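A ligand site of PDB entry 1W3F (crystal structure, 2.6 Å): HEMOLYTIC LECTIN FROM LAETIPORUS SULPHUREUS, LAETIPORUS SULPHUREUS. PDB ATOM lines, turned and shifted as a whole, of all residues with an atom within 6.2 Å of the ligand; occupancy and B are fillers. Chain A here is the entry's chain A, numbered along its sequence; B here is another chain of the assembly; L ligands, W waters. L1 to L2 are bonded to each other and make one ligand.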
ATOM      1  N   ARG A  76     -17.477 -14.541  17.128  1.00  0.00           N
ATOM      2  CA  ARG A  76     -17.724 -15.807  16.460  1.00  0.00           C
ATOM      3  C   ARG A  76     -18.629 -16.757  17.218  1.00  0.00           C
ATOM      4  O   ARG A  76     -19.447 -17.471  16.621  1.00  0.00           O
ATOM      5  CB  ARG A  76     -16.408 -16.513  16.109  1.00  0.00           C
ATOM      6  CG  ARG A  76     -16.030 -16.295  14.670  1.00  0.00           C
ATOM      7  CD  ARG A  76     -17.142 -16.765  13.755  1.00  0.00           C
ATOM      8  NE  ARG A  76     -17.100 -16.117  12.456  1.00  0.00           N
ATOM      9  CZ  ARG A  76     -17.723 -16.579  11.373  1.00  0.00           C
ATOM     10  NH1 ARG A  76     -18.431 -17.690  11.450  1.00  0.00           N
ATOM     11  NH2 ARG A  76     -17.640 -15.927  10.227  1.00  0.00           N
ATOM     12  N   GLU A  79     -24.553 -15.595  18.115  1.00  0.00           N
ATOM     13  CA  GLU A  79     -25.207 -15.098  16.916  1.00  0.00           C
ATOM     14  C   GLU A  79     -26.125 -13.937  17.290  1.00  0.00           C
ATOM     15  O   GLU A  79     -26.762 -13.956  18.346  1.00  0.00           O
ATOM     16  CB  GLU A  79     -26.022 -16.218  16.275  1.00  0.00           C
ATOM     17  CG  GLU A  79     -26.155 -16.125  14.768  1.00  0.00           C
ATOM     18  CD  GLU A  79     -24.885 -16.530  14.043  1.00  0.00           C
ATOM     19  OE1 GLU A  79     -24.513 -17.731  14.098  1.00  0.00           O
ATOM     20  OE2 GLU A  79     -24.253 -15.659  13.417  1.00  0.00           O
ATOM     21  N   TYR A  81     -23.169 -12.693  14.488  1.00  0.00           N
ATOM     22  CA  TYR A  81     -21.755 -12.363  14.629  1.00  0.00           C
ATOM     23  C   TYR A  81     -21.418 -10.870  14.617  1.00  0.00           C
ATOM     24  O   TYR A  81     -20.362 -10.481  15.104  1.00  0.00           O
ATOM     25  CB  TYR A  81     -20.931 -13.101  13.579  1.00  0.00           C
ATOM     26  CG  TYR A  81     -21.106 -14.601  13.610  1.00  0.00           C
ATOM     27  CD1 TYR A  81     -21.523 -15.259  14.764  1.00  0.00           C
ATOM     28  CD2 TYR A  81     -20.834 -15.374  12.476  1.00  0.00           C
ATOM     29  CE1 TYR A  81     -21.677 -16.646  14.790  1.00  0.00           C
ATOM     30  CE2 TYR A  81     -20.980 -16.754  12.500  1.00  0.00           C
ATOM     31  CZ  TYR A  81     -21.402 -17.375  13.654  1.00  0.00           C
ATOM     32  OH  TYR A  81     -21.563 -18.744  13.665  1.00  0.00           O
ATOM     33  N   LEU A 120     -14.336  -7.983   9.594  1.00  0.00           N
ATOM     34  CA  LEU A 120     -15.611  -7.536   9.045  1.00  0.00           C
ATOM     35  C   LEU A 120     -15.723  -7.834   7.557  1.00  0.00           C
ATOM     36  O   LEU A 120     -14.737  -7.763   6.818  1.00  0.00           O
ATOM     37  CB  LEU A 120     -15.841  -6.048   9.309  1.00  0.00           C
ATOM     38  CG  LEU A 120     -16.214  -5.709  10.755  1.00  0.00           C
ATOM     39  CD1 LEU A 120     -16.499  -4.238  10.871  1.00  0.00           C
ATOM     40  CD2 LEU A 120     -17.417  -6.536  11.189  1.00  0.00           C
ATOM     41  N   VAL A 121     -16.941  -8.151   7.148  1.00  0.00           N
ATOM     42  CA  VAL A 121     -17.249  -8.484   5.763  1.00  0.00           C
ATOM     43  C   VAL A 121     -18.322  -7.564   5.181  1.00  0.00           C
ATOM     44  O   VAL A 121     -19.318  -7.239   5.861  1.00  0.00           O
ATOM     45  CB  VAL A 121     -17.741  -9.963   5.663  1.00  0.00           C
ATOM     46  CG1 VAL A 121     -18.214 -10.273   4.253  1.00  0.00           C
ATOM     47  CG2 VAL A 121     -16.636 -10.913   6.083  1.00  0.00           C
ATOM     48  N   ARG A 123     -20.216  -7.479   1.468  1.00  0.00           N
ATOM     49  CA  ARG A 123     -20.423  -8.039   0.126  1.00  0.00           C
ATOM     50  C   ARG A 123     -21.891  -8.016  -0.303  1.00  0.00           C
ATOM     51  O   ARG A 123     -22.787  -7.862   0.526  1.00  0.00           O
ATOM     52  CB  ARG A 123     -19.974  -9.499   0.135  1.00  0.00           C
ATOM     53  CG  ARG A 123     -20.848 -10.335   1.055  1.00  0.00           C
ATOM     54  CD  ARG A 123     -20.202 -11.627   1.488  1.00  0.00           C
ATOM     55  NE  ARG A 123     -20.976 -12.210   2.579  1.00  0.00           N
ATOM     56  CZ  ARG A 123     -20.673 -13.341   3.204  1.00  0.00           C
ATOM     57  NH1 ARG A 123     -19.607 -14.052   2.864  1.00  0.00           N
ATOM     58  NH2 ARG A 123     -21.464 -13.767   4.193  1.00  0.00           N
ATOM     59  N   HIS A 125     -22.743 -10.338  -2.966  1.00  0.00           N
ATOM     60  CA  HIS A 125     -22.851 -11.600  -3.704  1.00  0.00           C
ATOM     61  C   HIS A 125     -23.313 -12.770  -2.836  1.00  0.00           C
ATOM     62  O   HIS A 125     -23.709 -13.818  -3.362  1.00  0.00           O
ATOM     63  CB  HIS A 125     -21.491 -11.939  -4.344  1.00  0.00           C
ATOM     64  CG  HIS A 125     -20.453 -12.390  -3.364  1.00  0.00           C
ATOM     65  ND1 HIS A 125     -20.124 -13.719  -3.192  1.00  0.00           N
ATOM     66  CD2 HIS A 125     -19.673 -11.699  -2.501  1.00  0.00           C
ATOM     67  CE1 HIS A 125     -19.196 -13.825  -2.255  1.00  0.00           C
ATOM     68  NE2 HIS A 125     -18.906 -12.609  -1.818  1.00  0.00           N
ATOM     69  N   LEU A 126     -23.270 -12.608  -1.520  1.00  0.00           N
ATOM     70  CA  LEU A 126     -23.637 -13.684  -0.608  1.00  0.00           C
ATOM     71  C   LEU A 126     -24.150 -13.105   0.705  1.00  0.00           C
ATOM     72  O   LEU A 126     -23.692 -12.062   1.152  1.00  0.00           O
ATOM     73  CB  LEU A 126     -22.406 -14.565  -0.384  1.00  0.00           C
ATOM     74  CG  LEU A 126     -22.388 -15.838   0.466  1.00  0.00           C
ATOM     75  CD1 LEU A 126     -22.464 -15.461   1.920  1.00  0.00           C
ATOM     76  CD2 LEU A 126     -23.523 -16.759   0.073  1.00  0.00           C
ATOM     77  N   GLN A 127     -25.128 -13.773   1.316  1.00  0.00           N
ATOM     78  CA  GLN A 127     -25.699 -13.310   2.595  1.00  0.00           C
ATOM     79  C   GLN A 127     -25.131 -14.053   3.789  1.00  0.00           C
ATOM     80  O   GLN A 127     -24.771 -15.228   3.695  1.00  0.00           O
ATOM     81  CB  GLN A 127     -27.218 -13.471   2.595  1.00  0.00           C
ATOM     82  CG  GLN A 127     -27.961 -12.503   1.707  1.00  0.00           C
ATOM     83  CD  GLN A 127     -29.453 -12.678   1.805  1.00  0.00           C
ATOM     84  OE1 GLN A 127     -30.229 -11.937   1.188  1.00  0.00           O
ATOM     85  NE2 GLN A 127     -29.892 -13.656   2.582  1.00  0.00           N
ATOM     86  N   PRO A 128     -25.045 -13.371   4.947  1.00  0.00           N
ATOM     87  CA  PRO A 128     -25.457 -11.964   5.135  1.00  0.00           C
ATOM     88  C   PRO A 128     -24.485 -11.027   4.432  1.00  0.00           C
ATOM     89  O   PRO A 128     -23.282 -11.294   4.349  1.00  0.00           O
ATOM     90  CB  PRO A 128     -25.419 -11.791   6.652  1.00  0.00           C
ATOM     91  CG  PRO A 128     -25.579 -13.187   7.184  1.00  0.00           C
ATOM     92  CD  PRO A 128     -24.720 -13.990   6.238  1.00  0.00           C
ATOM     93  N   TRP A 131     -21.307  -9.059   7.464  1.00  0.00           N
ATOM     94  CA  TRP A 131     -21.023 -10.167   8.369  1.00  0.00           C
ATOM     95  C   TRP A 131     -19.539 -10.128   8.713  1.00  0.00           C
ATOM     96  O   TRP A 131     -18.918  -9.081   8.618  1.00  0.00           O
ATOM     97  CB  TRP A 131     -21.339 -11.474   7.623  1.00  0.00           C
ATOM     98  CG  TRP A 131     -21.781 -12.609   8.478  1.00  0.00           C
ATOM     99  CD1 TRP A 131     -21.310 -13.896   8.428  1.00  0.00           C
ATOM    100  CD2 TRP A 131     -22.822 -12.600   9.449  1.00  0.00           C
ATOM    101  NE1 TRP A 131     -21.994 -14.679   9.320  1.00  0.00           N
ATOM    102  CE2 TRP A 131     -22.939 -13.912   9.957  1.00  0.00           C
ATOM    103  CE3 TRP A 131     -23.679 -11.608   9.947  1.00  0.00           C
ATOM    104  CZ2 TRP A 131     -23.865 -14.265  10.940  1.00  0.00           C
ATOM    105  CZ3 TRP A 131     -24.614 -11.951  10.926  1.00  0.00           C
ATOM    106  CH2 TRP A 131     -24.698 -13.263  11.405  1.00  0.00           C
ATOM    107  N   ASN A 132     -18.990 -11.261   9.154  1.00  0.00           N
ATOM    108  CA  ASN A 132     -17.563 -11.319   9.434  1.00  0.00           C
ATOM    109  C   ASN A 132     -17.003 -12.666   9.001  1.00  0.00           C
ATOM    110  O   ASN A 132     -17.745 -13.535   8.569  1.00  0.00           O
ATOM    111  CB  ASN A 132     -17.210 -11.036  10.910  1.00  0.00           C
ATOM    112  CG  ASN A 132     -17.658 -12.130  11.870  1.00  0.00           C
ATOM    113  OD1 ASN A 132     -17.722 -13.310  11.521  1.00  0.00           O
ATOM    114  ND2 ASN A 132     -17.933 -11.722  13.110  1.00  0.00           N
ATOM    115  N   HIS A 133     -15.690 -12.827   9.096  1.00  0.00           N
ATOM    116  CA  HIS A 133     -15.025 -14.036   8.643  1.00  0.00           C
ATOM    117  C   HIS A 133     -13.769 -14.283   9.493  1.00  0.00           C
ATOM    118  O   HIS A 133     -13.235 -13.360  10.113  1.00  0.00           O
ATOM    119  CB  HIS A 133     -14.643 -13.850   7.172  1.00  0.00           C
ATOM    120  CG  HIS A 133     -14.305 -15.115   6.459  1.00  0.00           C
ATOM    121  ND1 HIS A 133     -15.249 -16.078   6.175  1.00  0.00           N
ATOM    122  CD2 HIS A 133     -13.131 -15.570   5.954  1.00  0.00           C
ATOM    123  CE1 HIS A 133     -14.671 -17.081   5.530  1.00  0.00           C
ATOM    124  NE2 HIS A 133     -13.388 -16.792   5.383  1.00  0.00           N
ATOM    125  N   GLU A 137      -8.325 -16.028   6.905  1.00  0.00           N
ATOM    126  CA  GLU A 137      -8.641 -16.189   5.497  1.00  0.00           C
ATOM    127  C   GLU A 137      -9.031 -14.815   4.930  1.00  0.00           C
ATOM    128  O   GLU A 137     -10.132 -14.330   5.175  1.00  0.00           O
ATOM    129  CB  GLU A 137      -9.810 -17.159   5.304  1.00  0.00           C
ATOM    130  CG  GLU A 137      -9.438 -18.455   4.612  1.00  0.00           C
ATOM    131  CD  GLU A 137     -10.562 -18.989   3.745  1.00  0.00           C
ATOM    132  OE1 GLU A 137     -11.693 -19.114   4.246  1.00  0.00           O
ATOM    133  OE2 GLU A 137     -10.319 -19.282   2.549  1.00  0.00           O
ATOM    134  N   VAL A 138      -8.136 -14.212   4.173  1.00  0.00           N
ATOM    135  CA  VAL A 138      -8.377 -12.898   3.608  1.00  0.00           C
ATOM    136  C   VAL A 138      -9.010 -12.880   2.211  1.00  0.00           C
ATOM    137  O   VAL A 138      -8.471 -13.458   1.266  1.00  0.00           O
ATOM    138  CB  VAL A 138      -7.056 -12.083   3.535  1.00  0.00           C
ATOM    139  CG1 VAL A 138      -7.341 -10.655   3.158  1.00  0.00           C
ATOM    140  CG2 VAL A 138      -6.335 -12.143   4.877  1.00  0.00           C
ATOM    141  N   PHE A 139     -10.154 -12.215   2.108  1.00  0.00           N
ATOM    142  CA  PHE A 139     -10.877 -12.050   0.840  1.00  0.00           C
ATOM    143  C   PHE A 139     -11.063 -10.561   0.611  1.00  0.00           C
ATOM    144  O   PHE A 139     -11.127  -9.777   1.560  1.00  0.00           O
ATOM    145  CB  PHE A 139     -12.251 -12.721   0.882  1.00  0.00           C
ATOM    146  CG  PHE A 139     -12.217 -14.216   0.763  1.00  0.00           C
ATOM    147  CD1 PHE A 139     -12.214 -15.019   1.897  1.00  0.00           C
ATOM    148  CD2 PHE A 139     -12.241 -14.813  -0.487  1.00  0.00           C
ATOM    149  CE1 PHE A 139     -12.244 -16.409   1.778  1.00  0.00           C
ATOM    150  CE2 PHE A 139     -12.264 -16.202  -0.621  1.00  0.00           C
ATOM    151  CZ  PHE A 139     -12.260 -17.005   0.513  1.00  0.00           C
ATOM    152  N   ASP A 140     -11.169 -10.150  -0.648  1.00  0.00           N
ATOM    153  CA  ASP A 140     -11.345  -8.739  -0.982  1.00  0.00           C
ATOM    154  C   ASP A 140     -12.553  -8.066  -0.360  1.00  0.00           C
ATOM    155  O   ASP A 140     -12.543  -6.854  -0.148  1.00  0.00           O
ATOM    156  CB  ASP A 140     -11.416  -8.551  -2.508  1.00  0.00           C
ATOM    157  CG  ASP A 140     -10.057  -8.475  -3.161  1.00  0.00           C
ATOM    158  OD1 ASP A 140      -9.047  -8.312  -2.441  1.00  0.00           O
ATOM    159  OD2 ASP A 140      -9.987  -8.557  -4.412  1.00  0.00           O
ATOM    160  N   ASP A 141     -13.604  -8.831  -0.057  1.00  0.00           N
ATOM    161  CA  ASP A 141     -14.797  -8.239   0.514  1.00  0.00           C
ATOM    162  C   ASP A 141     -14.670  -7.875   1.975  1.00  0.00           C
ATOM    163  O   ASP A 141     -15.654  -7.540   2.629  1.00  0.00           O
ATOM    164  CB  ASP A 141     -16.034  -9.138   0.304  1.00  0.00           C
ATOM    165  CG  ASP A 141     -15.834 -10.570   0.792  1.00  0.00           C
ATOM    166  OD1 ASP A 141     -14.951 -10.823   1.647  1.00  0.00           O
ATOM    167  OD2 ASP A 141     -16.584 -11.445   0.317  1.00  0.00           O
ATOM    168  N   GLN A 142     -13.452  -7.944   2.485  1.00  0.00           N
ATOM    169  CA  GLN A 142     -13.160  -7.607   3.867  1.00  0.00           C
ATOM    170  C   GLN A 142     -12.559  -6.205   3.928  1.00  0.00           C
ATOM    171  O   GLN A 142     -12.239  -5.692   5.005  1.00  0.00           O
ATOM    172  CB  GLN A 142     -12.162  -8.611   4.456  1.00  0.00           C
ATOM    173  CG  GLN A 142     -12.804  -9.888   4.999  1.00  0.00           C
ATOM    174  CD  GLN A 142     -11.830 -11.057   5.065  1.00  0.00           C
ATOM    175  OE1 GLN A 142     -10.680 -10.900   5.459  1.00  0.00           O
ATOM    176  NE2 GLN A 142     -12.291 -12.227   4.691  1.00  0.00           N
ATOM    177  N   SER B  37     -15.132 -16.293  -7.454  1.00  0.00           N
ATOM    178  CA  SER B  37     -14.857 -15.983  -6.070  1.00  0.00           C
ATOM    179  C   SER B  37     -14.105 -14.687  -5.860  1.00  0.00           C
ATOM    180  O   SER B  37     -13.313 -14.262  -6.712  1.00  0.00           O
ATOM    181  CB  SER B  37     -14.029 -17.100  -5.423  1.00  0.00           C
ATOM    182  OG  SER B  37     -13.479 -16.643  -4.189  1.00  0.00           O
ATOM    183  N   PRO B  38     -14.362 -14.026  -4.728  1.00  0.00           N
ATOM    184  CA  PRO B  38     -13.682 -12.771  -4.422  1.00  0.00           C
ATOM    185  C   PRO B  38     -12.214 -13.189  -4.286  1.00  0.00           C
ATOM    186  O   PRO B  38     -11.933 -14.347  -3.955  1.00  0.00           O
ATOM    187  CB  PRO B  38     -14.278 -12.365  -3.075  1.00  0.00           C
ATOM    188  CG  PRO B  38     -15.655 -12.955  -3.126  1.00  0.00           C
ATOM    189  CD  PRO B  38     -15.412 -14.310  -3.732  1.00  0.00           C
HETATM  190  C1  LIG L   1     -20.454 -19.655   6.024  1.00  0.00           C
HETATM  191  C2  LIG L   1     -20.507 -18.081   6.081  1.00  0.00           C
HETATM  192  C3  LIG L   1     -20.099 -17.571   4.688  1.00  0.00           C
HETATM  193  C4  LIG L   1     -18.686 -18.051   4.320  1.00  0.00           C
HETATM  194  C5  LIG L   1     -18.594 -19.638   4.400  1.00  0.00           C
HETATM  195  C6  LIG L   1     -17.206 -20.251   4.518  1.00  0.00           C
HETATM  196  C7  LIG L   1     -22.259 -17.506   7.704  1.00  0.00           C
HETATM  197  C8  LIG L   1     -23.696 -17.034   7.875  1.00  0.00           C
HETATM  198  O1  LIG L   1     -19.136 -20.040   5.659  1.00  0.00           O
HETATM  199  O2  LIG L   1     -20.119 -16.152   4.633  1.00  0.00           O
HETATM  200  O3  LIG L   1     -18.416 -17.560   3.004  1.00  0.00           O
HETATM  201  O4  LIG L   1     -16.493 -20.011   3.454  1.00  0.00           O
HETATM  202  O5  LIG L   1     -21.519 -17.766   8.699  1.00  0.00           O
HETATM  203  N1  LIG L   1     -21.850 -17.630   6.418  1.00  0.00           N
HETATM  204  O6  LIG L   1     -21.357 -20.179   5.104  1.00  0.00           O
HETATM  205  C1  LG2 L   2     -17.396 -16.750   2.636  1.00  0.00           C
HETATM  206  C2  LG2 L   2     -17.401 -16.687   1.056  1.00  0.00           C
HETATM  207  C3  LG2 L   2     -16.291 -15.760   0.464  1.00  0.00           C
HETATM  208  C4  LG2 L   2     -16.157 -14.446   1.258  1.00  0.00           C
HETATM  209  C5  LG2 L   2     -16.014 -14.733   2.782  1.00  0.00           C
HETATM  210  C6  LG2 L   2     -15.864 -13.446   3.596  1.00  0.00           C
HETATM  211  O1  LG2 L   2     -17.241 -17.978   0.450  1.00  0.00           O
HETATM  212  O2  LG2 L   2     -16.599 -15.465  -0.904  1.00  0.00           O
HETATM  213  O3  LG2 L   2     -17.310 -13.657   1.029  1.00  0.00           O
HETATM  214  O4  LG2 L   2     -17.142 -15.477   3.255  1.00  0.00           O
HETATM  215  O5  LG2 L   2     -14.578 -12.917   3.483  1.00  0.00           O
HETATM  216  O   HOH W   1     -19.467 -19.622  -0.253  1.00  0.00           O
HETATM  217  O   HOH W   2     -23.772 -17.731   4.088  1.00  0.00           O
HETATM  218  O   HOH W   3     -17.757 -15.660   6.754  1.00  0.00           O
HETATM  219  O   HOH W   4     -15.456 -17.649  -2.208  1.00  0.00           O
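ND2 of Asn 132 lies close to O of Tyr 81, at 3.4 Å. NE of Arg 123 is in hydrogen-bond range of O of Pro 128 (3.0 Å). N of Val 121 is in hydrogen-bond range of O of Trp 131, at 2.6 Å. The side-chain carboxylate (OE1) of Glu 79 lies close to the side-chain hydroxyl (OH) of Tyr 81, 3.1 Å away. NE of Arg 123 is in hydrogen-bond range of O of Leu 126, at 3.1 Å. NE2 of His 133 lies within hydrogen-bond range of OE1 of Glu 137. O of Glu 137 sits at hydrogen-bond distance from NE2 of Gln 142 (3.1 Å). OD2 of Asp 141 sits at hydrogen-bond distance from NE2 of His 125.
Water W4 bridges O2 of LG2 L2 and OG of Ser 37 of chain B. Water W2 lies within hydrogen-bond range of the backbone carbonyl oxygen of Gln 127 and a nitrogen (N1) of LIG L1. Water W3 lies within hydrogen-bond range of ND1 of His 133 (2.6 Å), O of Asn 132 (2.8 Å), O2 of LIG L1 (3.2 Å) and NH2 of Arg 76 (3.5 Å).
The side-chain amide nitrogen (NE2) of Gln 142 sits at hydrogen-bond distance from an oxygen (O5) of LG2 L2 (2.7 Å). The indole nitrogen (NE1) of Trp 131 lies within hydrogen-bond range of an oxygen (O5) of LIG L1 (3.2 Å). The guanidinium group (NH2) of Arg 123 lies within hydrogen-bond range of an oxygen (O2) of LIG L1 (2.8 Å). The side-chain carboxylate (OD2) of Asp 141 lies within hydrogen-bond range of an oxygen (O3) of LG2 L2, 2.4 Å away. A ring nitrogen (NE2) of His 125 lies within hydrogen-bond range of an oxygen (O3) of LG2 L2 (3.4 Å).
Tyr 81 touches the ligand. Val 121 touches the ligand. CD1 of Leu 126 touches O2 of LIG L1, 3.7 Å away. Pro 128 touches the ligand. His 133 touches the ligand. CB of Phe 139 touches O5 of LG2 L2, 3.5 Å away. Pro 38 of chain B touches the ligand. Hydrophobic or aromatic side chains within 4 Å of the ligand: Tyr 81, Val 121, His 125, Leu 126, Pro 128, Trp 131, His 133, Phe 139 and Pro 38 of chain B. Of the 21 residues printed, 12 come within 4 Å of the ligand.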
